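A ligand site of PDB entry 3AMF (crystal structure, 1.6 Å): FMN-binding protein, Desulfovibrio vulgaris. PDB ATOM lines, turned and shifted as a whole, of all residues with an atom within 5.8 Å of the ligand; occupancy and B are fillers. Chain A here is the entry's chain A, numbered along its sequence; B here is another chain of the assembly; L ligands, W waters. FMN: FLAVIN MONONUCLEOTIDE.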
ATOM      1  N   VAL A  15       8.394  10.291   7.027  1.00  0.00           N
ATOM      2  CA  VAL A  15       7.690  11.563   6.865  1.00  0.00           C
ATOM      3  C   VAL A  15       8.713  12.685   6.750  1.00  0.00           C
ATOM      4  O   VAL A  15       9.577  12.846   7.610  1.00  0.00           O
ATOM      5  CB  VAL A  15       6.733  11.823   8.061  1.00  0.00           C
ATOM      6  CG1 VAL A  15       6.099  13.206   7.958  1.00  0.00           C
ATOM      7  CG2 VAL A  15       5.661  10.731   8.135  1.00  0.00           C
ATOM      8  N   HIS A  27       5.085  28.026   9.133  1.00  0.00           N
ATOM      9  CA  HIS A  27       4.146  27.005   8.704  1.00  0.00           C
ATOM     10  C   HIS A  27       4.925  25.714   8.488  1.00  0.00           C
ATOM     11  O   HIS A  27       6.125  25.747   8.212  1.00  0.00           O
ATOM     12  CB  HIS A  27       3.396  27.416   7.436  1.00  0.00           C
ATOM     13  CG  HIS A  27       2.216  26.532   7.142  1.00  0.00           C
ATOM     14  ND1 HIS A  27       1.316  26.152   8.106  1.00  0.00           N
ATOM     15  CD2 HIS A  27       1.814  25.936   5.996  1.00  0.00           C
ATOM     16  CE1 HIS A  27       0.394  25.371   7.562  1.00  0.00           C
ATOM     17  NE2 HIS A  27       0.675  25.223   6.283  1.00  0.00           N
ATOM     18  N   LEU A  28       4.232  24.586   8.635  1.00  0.00           N
ATOM     19  CA  LEU A  28       4.873  23.283   8.555  1.00  0.00           C
ATOM     20  C   LEU A  28       3.973  22.302   7.835  1.00  0.00           C
ATOM     21  O   LEU A  28       2.817  22.099   8.235  1.00  0.00           O
ATOM     22  CB  LEU A  28       5.213  22.788   9.968  1.00  0.00           C
ATOM     23  CG  LEU A  28       6.060  21.528  10.135  1.00  0.00           C
ATOM     24  CD1 LEU A  28       7.431  21.703   9.523  1.00  0.00           C
ATOM     25  CD2 LEU A  28       6.165  21.180  11.611  1.00  0.00           C
ATOM     26  N   VAL A  29       4.498  21.707   6.757  1.00  0.00           N
ATOM     27  CA  VAL A  29       3.790  20.698   5.972  1.00  0.00           C
ATOM     28  C   VAL A  29       4.667  19.468   5.748  1.00  0.00           C
ATOM     29  O   VAL A  29       5.833  19.452   6.128  1.00  0.00           O
ATOM     30  CB  VAL A  29       3.267  21.271   4.622  1.00  0.00           C
ATOM     31  CG1 VAL A  29       2.313  22.431   4.870  1.00  0.00           C
ATOM     32  CG2 VAL A  29       4.427  21.684   3.692  1.00  0.00           C
ATOM     33  N   ASN A  30       4.086  18.461   5.103  1.00  0.00           N
ATOM     34  CA  ASN A  30       4.755  17.168   4.956  1.00  0.00           C
ATOM     35  C   ASN A  30       4.733  16.607   3.550  1.00  0.00           C
ATOM     36  O   ASN A  30       3.898  16.967   2.713  1.00  0.00           O
ATOM     37  CB  ASN A  30       4.112  16.142   5.897  1.00  0.00           C
ATOM     38  CG  ASN A  30       4.214  16.534   7.341  1.00  0.00           C
ATOM     39  OD1 ASN A  30       3.197  16.833   7.979  1.00  0.00           O
ATOM     40  ND2 ASN A  30       5.427  16.568   7.875  1.00  0.00           N
ATOM     41  N   THR A  31       5.665  15.687   3.304  1.00  0.00           N
ATOM     42  CA  THR A  31       5.570  14.755   2.206  1.00  0.00           C
ATOM     43  C   THR A  31       6.160  13.422   2.694  1.00  0.00           C
ATOM     44  O   THR A  31       6.387  13.246   3.893  1.00  0.00           O
ATOM     45  CB  THR A  31       6.212  15.312   0.891  1.00  0.00           C
ATOM     46  OG1 THR A  31       5.934  14.438  -0.205  1.00  0.00           O
ATOM     47  CG2 THR A  31       7.718  15.489   1.027  1.00  0.00           C
ATOM     48  N   TRP A  32       6.352  12.474   1.778  1.00  0.00           N
ATOM     49  CA  TRP A  32       6.945  11.191   2.113  1.00  0.00           C
ATOM     50  C   TRP A  32       8.378  11.137   1.602  1.00  0.00           C
ATOM     51  O   TRP A  32       8.683  11.719   0.561  1.00  0.00           O
ATOM     52  CB  TRP A  32       6.143  10.061   1.477  1.00  0.00           C
ATOM     53  CG  TRP A  32       4.711   9.925   1.927  1.00  0.00           C
ATOM     54  CD1 TRP A  32       3.589  10.191   1.182  1.00  0.00           C
ATOM     55  CD2 TRP A  32       4.253   9.461   3.199  1.00  0.00           C
ATOM     56  NE1 TRP A  32       2.457   9.939   1.934  1.00  0.00           N
ATOM     57  CE2 TRP A  32       2.835   9.484   3.168  1.00  0.00           C
ATOM     58  CE3 TRP A  32       4.895   9.039   4.375  1.00  0.00           C
ATOM     59  CZ2 TRP A  32       2.060   9.096   4.263  1.00  0.00           C
ATOM     60  CZ3 TRP A  32       4.119   8.651   5.460  1.00  0.00           C
ATOM     61  CH2 TRP A  32       2.715   8.685   5.397  1.00  0.00           C
ATOM     62  N   TYR A  35       8.757  10.348  -2.060  1.00  0.00           N
ATOM     63  CA  TYR A  35       8.225  11.291  -3.044  1.00  0.00           C
ATOM     64  C   TYR A  35       9.255  12.303  -3.526  1.00  0.00           C
ATOM     65  O   TYR A  35       9.038  12.999  -4.525  1.00  0.00           O
ATOM     66  CB  TYR A  35       6.995  12.018  -2.490  1.00  0.00           C
ATOM     67  CG  TYR A  35       5.724  11.183  -2.433  1.00  0.00           C
ATOM     68  CD1 TYR A  35       5.759   9.793  -2.557  1.00  0.00           C
ATOM     69  CD2 TYR A  35       4.503  11.799  -2.237  1.00  0.00           C
ATOM     70  CE1 TYR A  35       4.591   9.040  -2.488  1.00  0.00           C
ATOM     71  CE2 TYR A  35       3.333  11.056  -2.178  1.00  0.00           C
ATOM     72  CZ  TYR A  35       3.377   9.686  -2.303  1.00  0.00           C
ATOM     73  OH  TYR A  35       2.209   8.973  -2.234  1.00  0.00           O
ATOM     74  N   VAL A  46       9.522  18.015  -5.022  1.00  0.00           N
ATOM     75  CA  VAL A  46       8.405  17.443  -4.262  1.00  0.00           C
ATOM     76  C   VAL A  46       7.112  17.617  -5.057  1.00  0.00           C
ATOM     77  O   VAL A  46       6.841  18.714  -5.540  1.00  0.00           O
ATOM     78  CB  VAL A  46       8.245  18.172  -2.894  1.00  0.00           C
ATOM     79  CG1 VAL A  46       7.097  17.580  -2.078  1.00  0.00           C
ATOM     80  CG2 VAL A  46       9.547  18.138  -2.091  1.00  0.00           C
ATOM     81  N   PRO A  47       6.301  16.548  -5.173  1.00  0.00           N
ATOM     82  CA  PRO A  47       4.986  16.732  -5.812  1.00  0.00           C
ATOM     83  C   PRO A  47       4.040  17.532  -4.913  1.00  0.00           C
ATOM     84  O   PRO A  47       3.933  17.252  -3.715  1.00  0.00           O
ATOM     85  CB  PRO A  47       4.484  15.296  -5.982  1.00  0.00           C
ATOM     86  CG  PRO A  47       5.141  14.545  -4.858  1.00  0.00           C
ATOM     87  CD  PRO A  47       6.521  15.141  -4.771  1.00  0.00           C
ATOM     88  N   VAL A  48       3.333  18.494  -5.511  1.00  0.00           N
ATOM     89  CA  VAL A  48       2.441  19.384  -4.764  1.00  0.00           C
ATOM     90  C   VAL A  48       0.988  19.117  -5.123  1.00  0.00           C
ATOM     91  O   VAL A  48       0.587  19.292  -6.271  1.00  0.00           O
ATOM     92  CB  VAL A  48       2.782  20.868  -5.033  1.00  0.00           C
ATOM     93  CG1 VAL A  48       1.762  21.797  -4.375  1.00  0.00           C
ATOM     94  CG2 VAL A  48       4.179  21.194  -4.532  1.00  0.00           C
ATOM     95  N   GLY A  49       0.214  18.669  -4.140  1.00  0.00           N
ATOM     96  CA  GLY A  49      -1.235  18.522  -4.297  1.00  0.00           C
ATOM     97  C   GLY A  49      -1.927  19.705  -3.658  1.00  0.00           C
ATOM     98  O   GLY A  49      -2.720  20.395  -4.300  1.00  0.00           O
ATOM     99  N   GLY A  50      -1.620  19.940  -2.383  1.00  0.00           N
ATOM    100  CA  GLY A  50      -2.132  21.104  -1.655  1.00  0.00           C
ATOM    101  C   GLY A  50      -1.099  22.216  -1.599  1.00  0.00           C
ATOM    102  O   GLY A  50      -0.877  22.918  -2.586  1.00  0.00           O
ATOM    103  N   MET A  51      -0.465  22.355  -0.433  1.00  0.00           N
ATOM    104  CA  MET A  51       0.574  23.357  -0.185  1.00  0.00           C
ATOM    105  C   MET A  51       0.210  24.772  -0.652  1.00  0.00           C
ATOM    106  O   MET A  51       1.047  25.481  -1.210  1.00  0.00           O
ATOM    107  CB  MET A  51       1.921  22.902  -0.750  1.00  0.00           C
ATOM    108  CG  MET A  51       2.400  21.598  -0.141  1.00  0.00           C
ATOM    109  SD  MET A  51       4.139  21.297  -0.492  1.00  0.00           S
ATOM    110  CE  MET A  51       4.305  19.619   0.103  1.00  0.00           C
ATOM    111  N   HIS A  52      -1.031  25.188  -0.411  1.00  0.00           N
ATOM    112  CA  HIS A  52      -1.469  26.533  -0.783  1.00  0.00           C
ATOM    113  C   HIS A  52      -0.891  27.610   0.126  1.00  0.00           C
ATOM    114  O   HIS A  52      -0.419  28.646  -0.347  1.00  0.00           O
ATOM    115  CB  HIS A  52      -2.991  26.616  -0.826  1.00  0.00           C
ATOM    116  CG  HIS A  52      -3.595  25.808  -1.924  1.00  0.00           C
ATOM    117  ND1 HIS A  52      -3.551  26.197  -3.244  1.00  0.00           N
ATOM    118  CD2 HIS A  52      -4.239  24.610  -1.907  1.00  0.00           C
ATOM    119  CE1 HIS A  52      -4.153  25.290  -3.997  1.00  0.00           C
ATOM    120  NE2 HIS A  52      -4.580  24.315  -3.207  1.00  0.00           N
ATOM    121  N   LYS A  53      -0.907  27.361   1.440  1.00  0.00           N
ATOM    122  CA  LYS A  53      -0.323  28.309   2.379  1.00  0.00           C
ATOM    123  C   LYS A  53       1.203  28.306   2.218  1.00  0.00           C
ATOM    124  O   LYS A  53       1.834  29.364   2.234  1.00  0.00           O
ATOM    125  CB  LYS A  53      -0.721  27.975   3.823  1.00  0.00           C
ATOM    126  CG  LYS A  53      -2.184  28.249   4.125  1.00  0.00           C
ATOM    127  CD  LYS A  53      -2.533  27.936   5.560  1.00  0.00           C
ATOM    128  CE  LYS A  53      -4.037  27.999   5.788  1.00  0.00           C
ATOM    129  NZ  LYS A  53      -4.410  27.486   7.136  1.00  0.00           N
ATOM    130  N   THR A  54       1.763  27.112   2.040  1.00  0.00           N
ATOM    131  CA  THR A  54       3.191  26.939   1.775  1.00  0.00           C
ATOM    132  C   THR A  54       3.654  27.723   0.552  1.00  0.00           C
ATOM    133  O   THR A  54       4.681  28.405   0.599  1.00  0.00           O
ATOM    134  CB  THR A  54       3.554  25.442   1.663  1.00  0.00           C
ATOM    135  OG1 THR A  54       3.267  24.810   2.915  1.00  0.00           O
ATOM    136  CG2 THR A  54       5.035  25.229   1.297  1.00  0.00           C
ATOM    137  N   GLU A  55       2.900  27.633  -0.542  1.00  0.00           N
ATOM    138  CA  GLU A  55       3.240  28.356  -1.774  1.00  0.00           C
ATOM    139  C   GLU A  55       3.180  29.866  -1.564  1.00  0.00           C
ATOM    140  O   GLU A  55       4.079  30.576  -2.001  1.00  0.00           O
ATOM    141  CB  GLU A  55       2.325  27.945  -2.940  1.00  0.00           C
ATOM    142  CG  GLU A  55       2.661  28.658  -4.251  1.00  0.00           C
ATOM    143  CD  GLU A  55       1.787  28.247  -5.414  1.00  0.00           C
ATOM    144  OE1 GLU A  55       0.813  27.486  -5.228  1.00  0.00           O
ATOM    145  OE2 GLU A  55       2.078  28.699  -6.544  1.00  0.00           O
ATOM    146  N   TRP A 106      -2.112  13.528  -9.114  1.00  0.00           N
ATOM    147  CA  TRP A 106      -2.747  14.501  -8.231  1.00  0.00           C
ATOM    148  C   TRP A 106      -1.941  15.791  -8.074  1.00  0.00           C
ATOM    149  O   TRP A 106      -2.425  16.756  -7.482  1.00  0.00           O
ATOM    150  CB  TRP A 106      -3.002  13.890  -6.852  1.00  0.00           C
ATOM    151  CG  TRP A 106      -1.835  13.133  -6.287  1.00  0.00           C
ATOM    152  CD1 TRP A 106      -1.600  11.786  -6.366  1.00  0.00           C
ATOM    153  CD2 TRP A 106      -0.734  13.687  -5.551  1.00  0.00           C
ATOM    154  NE1 TRP A 106      -0.435  11.470  -5.720  1.00  0.00           N
ATOM    155  CE2 TRP A 106       0.121  12.607  -5.213  1.00  0.00           C
ATOM    156  CE3 TRP A 106      -0.389  14.981  -5.129  1.00  0.00           C
ATOM    157  CZ2 TRP A 106       1.296  12.791  -4.480  1.00  0.00           C
ATOM    158  CZ3 TRP A 106       0.785  15.155  -4.405  1.00  0.00           C
ATOM    159  CH2 TRP A 106       1.617  14.065  -4.083  1.00  0.00           C
ATOM    160  N   LEU B  68       3.839  14.734  12.513  1.00  0.00           N
ATOM    161  CA  LEU B  68       4.222  13.338  12.631  1.00  0.00           C
ATOM    162  C   LEU B  68       3.293  12.517  11.764  1.00  0.00           C
ATOM    163  O   LEU B  68       2.207  12.984  11.398  1.00  0.00           O
ATOM    164  CB  LEU B  68       4.143  12.879  14.089  1.00  0.00           C
ATOM    165  CG  LEU B  68       2.800  12.884  14.817  1.00  0.00           C
ATOM    166  CD1 LEU B  68       2.840  11.865  15.941  1.00  0.00           C
ATOM    167  CD2 LEU B  68       2.432  14.270  15.347  1.00  0.00           C
ATOM    168  N   GLY B  69       3.704  11.311  11.429  1.00  0.00           N
ATOM    169  CA  GLY B  69       2.882  10.451  10.583  1.00  0.00           C
ATOM    170  C   GLY B  69       3.391   9.047  10.445  1.00  0.00           C
ATOM    171  O   GLY B  69       4.415   8.689  11.035  1.00  0.00           O
ATOM    172  N   SER B  70       2.681   8.248   9.661  1.00  0.00           N
ATOM    173  CA  SER B  70       3.065   6.872   9.393  1.00  0.00           C
ATOM    174  C   SER B  70       2.380   6.353   8.145  1.00  0.00           C
ATOM    175  O   SER B  70       1.185   6.549   7.952  1.00  0.00           O
ATOM    176  CB  SER B  70       2.696   5.969  10.569  1.00  0.00           C
ATOM    177  OG  SER B  70       3.055   4.622  10.275  1.00  0.00           O
ATOM    178  N   THR B  81      -1.087   8.313   6.952  1.00  0.00           N
ATOM    179  CA  THR B  81      -1.716   9.486   7.539  1.00  0.00           C
ATOM    180  C   THR B  81      -0.698  10.288   8.340  1.00  0.00           C
ATOM    181  O   THR B  81       0.423   9.851   8.557  1.00  0.00           O
ATOM    182  CB  THR B  81      -2.921   9.103   8.446  1.00  0.00           C
ATOM    183  OG1 THR B  81      -3.720  10.254   8.708  1.00  0.00           O
ATOM    184  CG2 THR B  81      -2.454   8.509   9.766  1.00  0.00           C
ATOM    185  N   GLY B  82      -1.122  11.474   8.768  1.00  0.00           N
ATOM    186  CA  GLY B  82      -0.290  12.304   9.612  1.00  0.00           C
ATOM    187  C   GLY B  82      -1.068  13.446  10.215  1.00  0.00           C
ATOM    188  O   GLY B  82      -2.249  13.662   9.877  1.00  0.00           O
ATOM    189  N   PHE B  83      -0.400  14.174  11.099  1.00  0.00           N
ATOM    190  CA  PHE B  83      -1.038  15.248  11.861  1.00  0.00           C
ATOM    191  C   PHE B  83      -0.188  16.497  11.918  1.00  0.00           C
ATOM    192  O   PHE B  83       1.041  16.432  11.973  1.00  0.00           O
ATOM    193  CB  PHE B  83      -1.315  14.786  13.293  1.00  0.00           C
ATOM    194  CG  PHE B  83      -2.392  13.763  13.397  1.00  0.00           C
ATOM    195  CD1 PHE B  83      -2.105  12.416  13.269  1.00  0.00           C
ATOM    196  CD2 PHE B  83      -3.717  14.158  13.623  1.00  0.00           C
ATOM    197  CE1 PHE B  83      -3.116  11.455  13.351  1.00  0.00           C
ATOM    198  CE2 PHE B  83      -4.726  13.207  13.715  1.00  0.00           C
ATOM    199  CZ  PHE B  83      -4.430  11.860  13.585  1.00  0.00           C
ATOM    200  N   THR B 121      -3.962  15.691   8.492  1.00  0.00           N
ATOM    201  CA  THR B 121      -3.688  16.373   7.232  1.00  0.00           C
ATOM    202  C   THR B 121      -3.606  15.413   6.042  1.00  0.00           C
ATOM    203  O   THR B 121      -3.376  15.835   4.912  1.00  0.00           O
ATOM    204  CB  THR B 121      -2.403  17.218   7.314  1.00  0.00           C
ATOM    205  OG1 THR B 121      -1.357  16.421   7.881  1.00  0.00           O
ATOM    206  CG2 THR B 121      -2.625  18.447   8.194  1.00  0.00           C
ATOM    207  N   LEU B 122      -3.796  14.121   6.313  1.00  0.00           N
ATOM    208  CA  LEU B 122      -3.840  13.110   5.267  1.00  0.00           C
ATOM    209  C   LEU B 122      -4.814  11.999   5.658  1.00  0.00           C
ATOM    210  O   LEU B 122      -4.916  11.639   6.825  1.00  0.00           O
ATOM    211  CB  LEU B 122      -2.439  12.536   4.998  1.00  0.00           C
ATOM    212  CG  LEU B 122      -2.253  11.577   3.819  1.00  0.00           C
ATOM    213  CD1 LEU B 122      -2.452  12.263   2.471  1.00  0.00           C
ATOM    214  CD2 LEU B 122      -0.884  10.923   3.881  1.00  0.00           C
ATOM    215  OXT LEU B 122      -5.527  11.440   4.822  1.00  0.00           O
HETATM  216  N1  FMN L   1       0.711  17.478   0.437  1.00  0.00           N
HETATM  217  C2  FMN L   1       1.265  17.674  -0.831  1.00  0.00           C
HETATM  218  O2  FMN L   1       0.953  18.660  -1.489  1.00  0.00           O
HETATM  219  N3  FMN L   1       2.176  16.754  -1.357  1.00  0.00           N
HETATM  220  C4  FMN L   1       2.533  15.628  -0.625  1.00  0.00           C
HETATM  221  O4  FMN L   1       3.351  14.837  -1.105  1.00  0.00           O
HETATM  222  C4A FMN L   1       1.981  15.423   0.643  1.00  0.00           C
HETATM  223  N5  FMN L   1       2.320  14.297   1.388  1.00  0.00           N
HETATM  224  C5A FMN L   1       1.983  14.235   2.738  1.00  0.00           C
HETATM  225  C6  FMN L   1       2.543  13.242   3.535  1.00  0.00           C
HETATM  226  C7  FMN L   1       2.207  13.179   4.886  1.00  0.00           C
HETATM  227  C7M FMN L   1       2.843  12.087   5.760  1.00  0.00           C
HETATM  228  C8  FMN L   1       1.308  14.099   5.430  1.00  0.00           C
HETATM  229  C8M FMN L   1       0.912  14.056   6.903  1.00  0.00           C
HETATM  230  C9  FMN L   1       0.737  15.082   4.625  1.00  0.00           C
HETATM  231  C9A FMN L   1       1.073  15.145   3.274  1.00  0.00           C
HETATM  232  N10 FMN L   1       0.527  16.158   2.445  1.00  0.00           N
HETATM  233  C10 FMN L   1       1.059  16.333   1.171  1.00  0.00           C
HETATM  234  C1' FMN L   1      -0.346  17.208   3.025  1.00  0.00           C
HETATM  235  C2' FMN L   1       0.507  18.459   3.387  1.00  0.00           C
HETATM  236  O2' FMN L   1       1.335  18.179   4.529  1.00  0.00           O
HETATM  237  C3' FMN L   1      -0.329  19.719   3.675  1.00  0.00           C
HETATM  238  O3' FMN L   1      -1.193  19.480   4.795  1.00  0.00           O
HETATM  239  C4' FMN L   1      -1.189  20.158   2.476  1.00  0.00           C
HETATM  240  O4' FMN L   1      -0.453  20.096   1.248  1.00  0.00           O
HETATM  241  C5' FMN L   1      -1.717  21.583   2.679  1.00  0.00           C
HETATM  242  O5' FMN L   1      -0.625  22.505   2.653  1.00  0.00           O
HETATM  243  P   FMN L   1      -0.758  24.014   3.140  1.00  0.00           P
HETATM  244  O1P FMN L   1      -1.160  23.971   4.695  1.00  0.00           O
HETATM  245  O2P FMN L   1      -1.995  24.679   2.344  1.00  0.00           O
HETATM  246  O3P FMN L   1       0.540  24.709   2.885  1.00  0.00           O
HETATM  247  O   HOH W   1      -2.131  16.454  -1.205  1.00  0.00           O
HETATM  248  O   HOH W   2       0.844  17.905   7.219  1.00  0.00           O
HETATM  249  O   HOH W   3      -3.353  24.677   5.939  1.00  0.00           O
HETATM  250  O   HOH W   4      -1.390  21.789   6.277  1.00  0.00           O
HETATM  251  O   HOH W   5       0.189  12.372  -0.135  1.00  0.00           O
HETATM  252  O   HOH W   6      -4.549  24.090   2.569  1.00  0.00           O
HETATM  253  O   HOH W   7      -3.874  18.669   4.292  1.00  0.00           O
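Water W3 lies within hydrogen-bond range of an oxygen (O1P) of the ligand (2.6 Å) and the side-chain amino group (NZ) of Lys 53 (3.2 Å).
Water W2 lies within hydrogen-bond range of the side-chain amide oxygen (OD1) of Asn 30, the side-chain hydroxyl (OG1) of Thr 121 of chain B and an oxygen (O2') of the ligand.
Water W7 lies within hydrogen-bond range of an oxygen (O3') of the ligand and the backbone carbonyl oxygen (O) of Thr 121 of chain B.
Residues that only touch the ligand: Thr 121 of chain B (3.4 Å), Trp 32 (3.4 Å), Tyr 35 (3.4 Å), Gly 82 of chain B (3.4 Å), Val 29 (3.5 Å), Trp 106 (3.5 Å), Val 48 (3.7 Å), Val 15 (3.9 Å) and Leu 122 of chain B (3.96 Å).
Hydrophobic or aromatic side chains that line the ligand: Val 15, His 27, Val 29, Trp 32, Tyr 35, Met 51, His 52, Trp 106 and Leu 122 of chain B.
The nearest printed residue that does not touch the ligand is Thr 81 of chain B (4.3 Å).
An oxygen (O3P) of the ligand lies within hydrogen-bond range of the backbone NH of Thr 54 (2.8 Å).
The side-chain hydroxyl (OG1) of Thr 54 sits at hydrogen-bond distance from an oxygen (O3P) of the ligand, at 2.7 Å.
A ring nitrogen (NE2) of His 27 sits at hydrogen-bond distance from an oxygen (O1P) of the ligand.
N of Gly 49 is in hydrogen-bond range of O2 of the ligand (2.8 Å).
O4 of the ligand sits at hydrogen-bond distance from OG1 of Thr 31 (2.8 Å).
N of Met 51 is in hydrogen-bond range of O4' of the ligand (2.8 Å).
N of Asn 30 is in hydrogen-bond range of O2' of the ligand (2.8 Å).
O2' of the ligand lies close to O of Asn 30 (3.4 Å).
The backbone NH (N) of His 52 is in hydrogen-bond range of an oxygen (O2P) of the ligand.
The backbone carbonyl oxygen (O) of Pro 47 sits at hydrogen-bond distance from a nitrogen (N3) of the ligand.
The backbone NH (N) of Gly 50 sits at hydrogen-bond distance from an oxygen (O2) of the ligand, at 3.0 Å.
An oxygen (O2P) of the ligand is in hydrogen-bond range of the backbone NH of Lys 53, 3.0 Å away.
N of Thr 121 of chain B sits at hydrogen-bond distance from O of Gly 82 of chain B (3.0 Å).
The side-chain hydroxyl of Thr 81 of chain B lies within hydrogen-bond range of the chain-end carboxylate of Leu 122 of chain B (2.6 Å).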
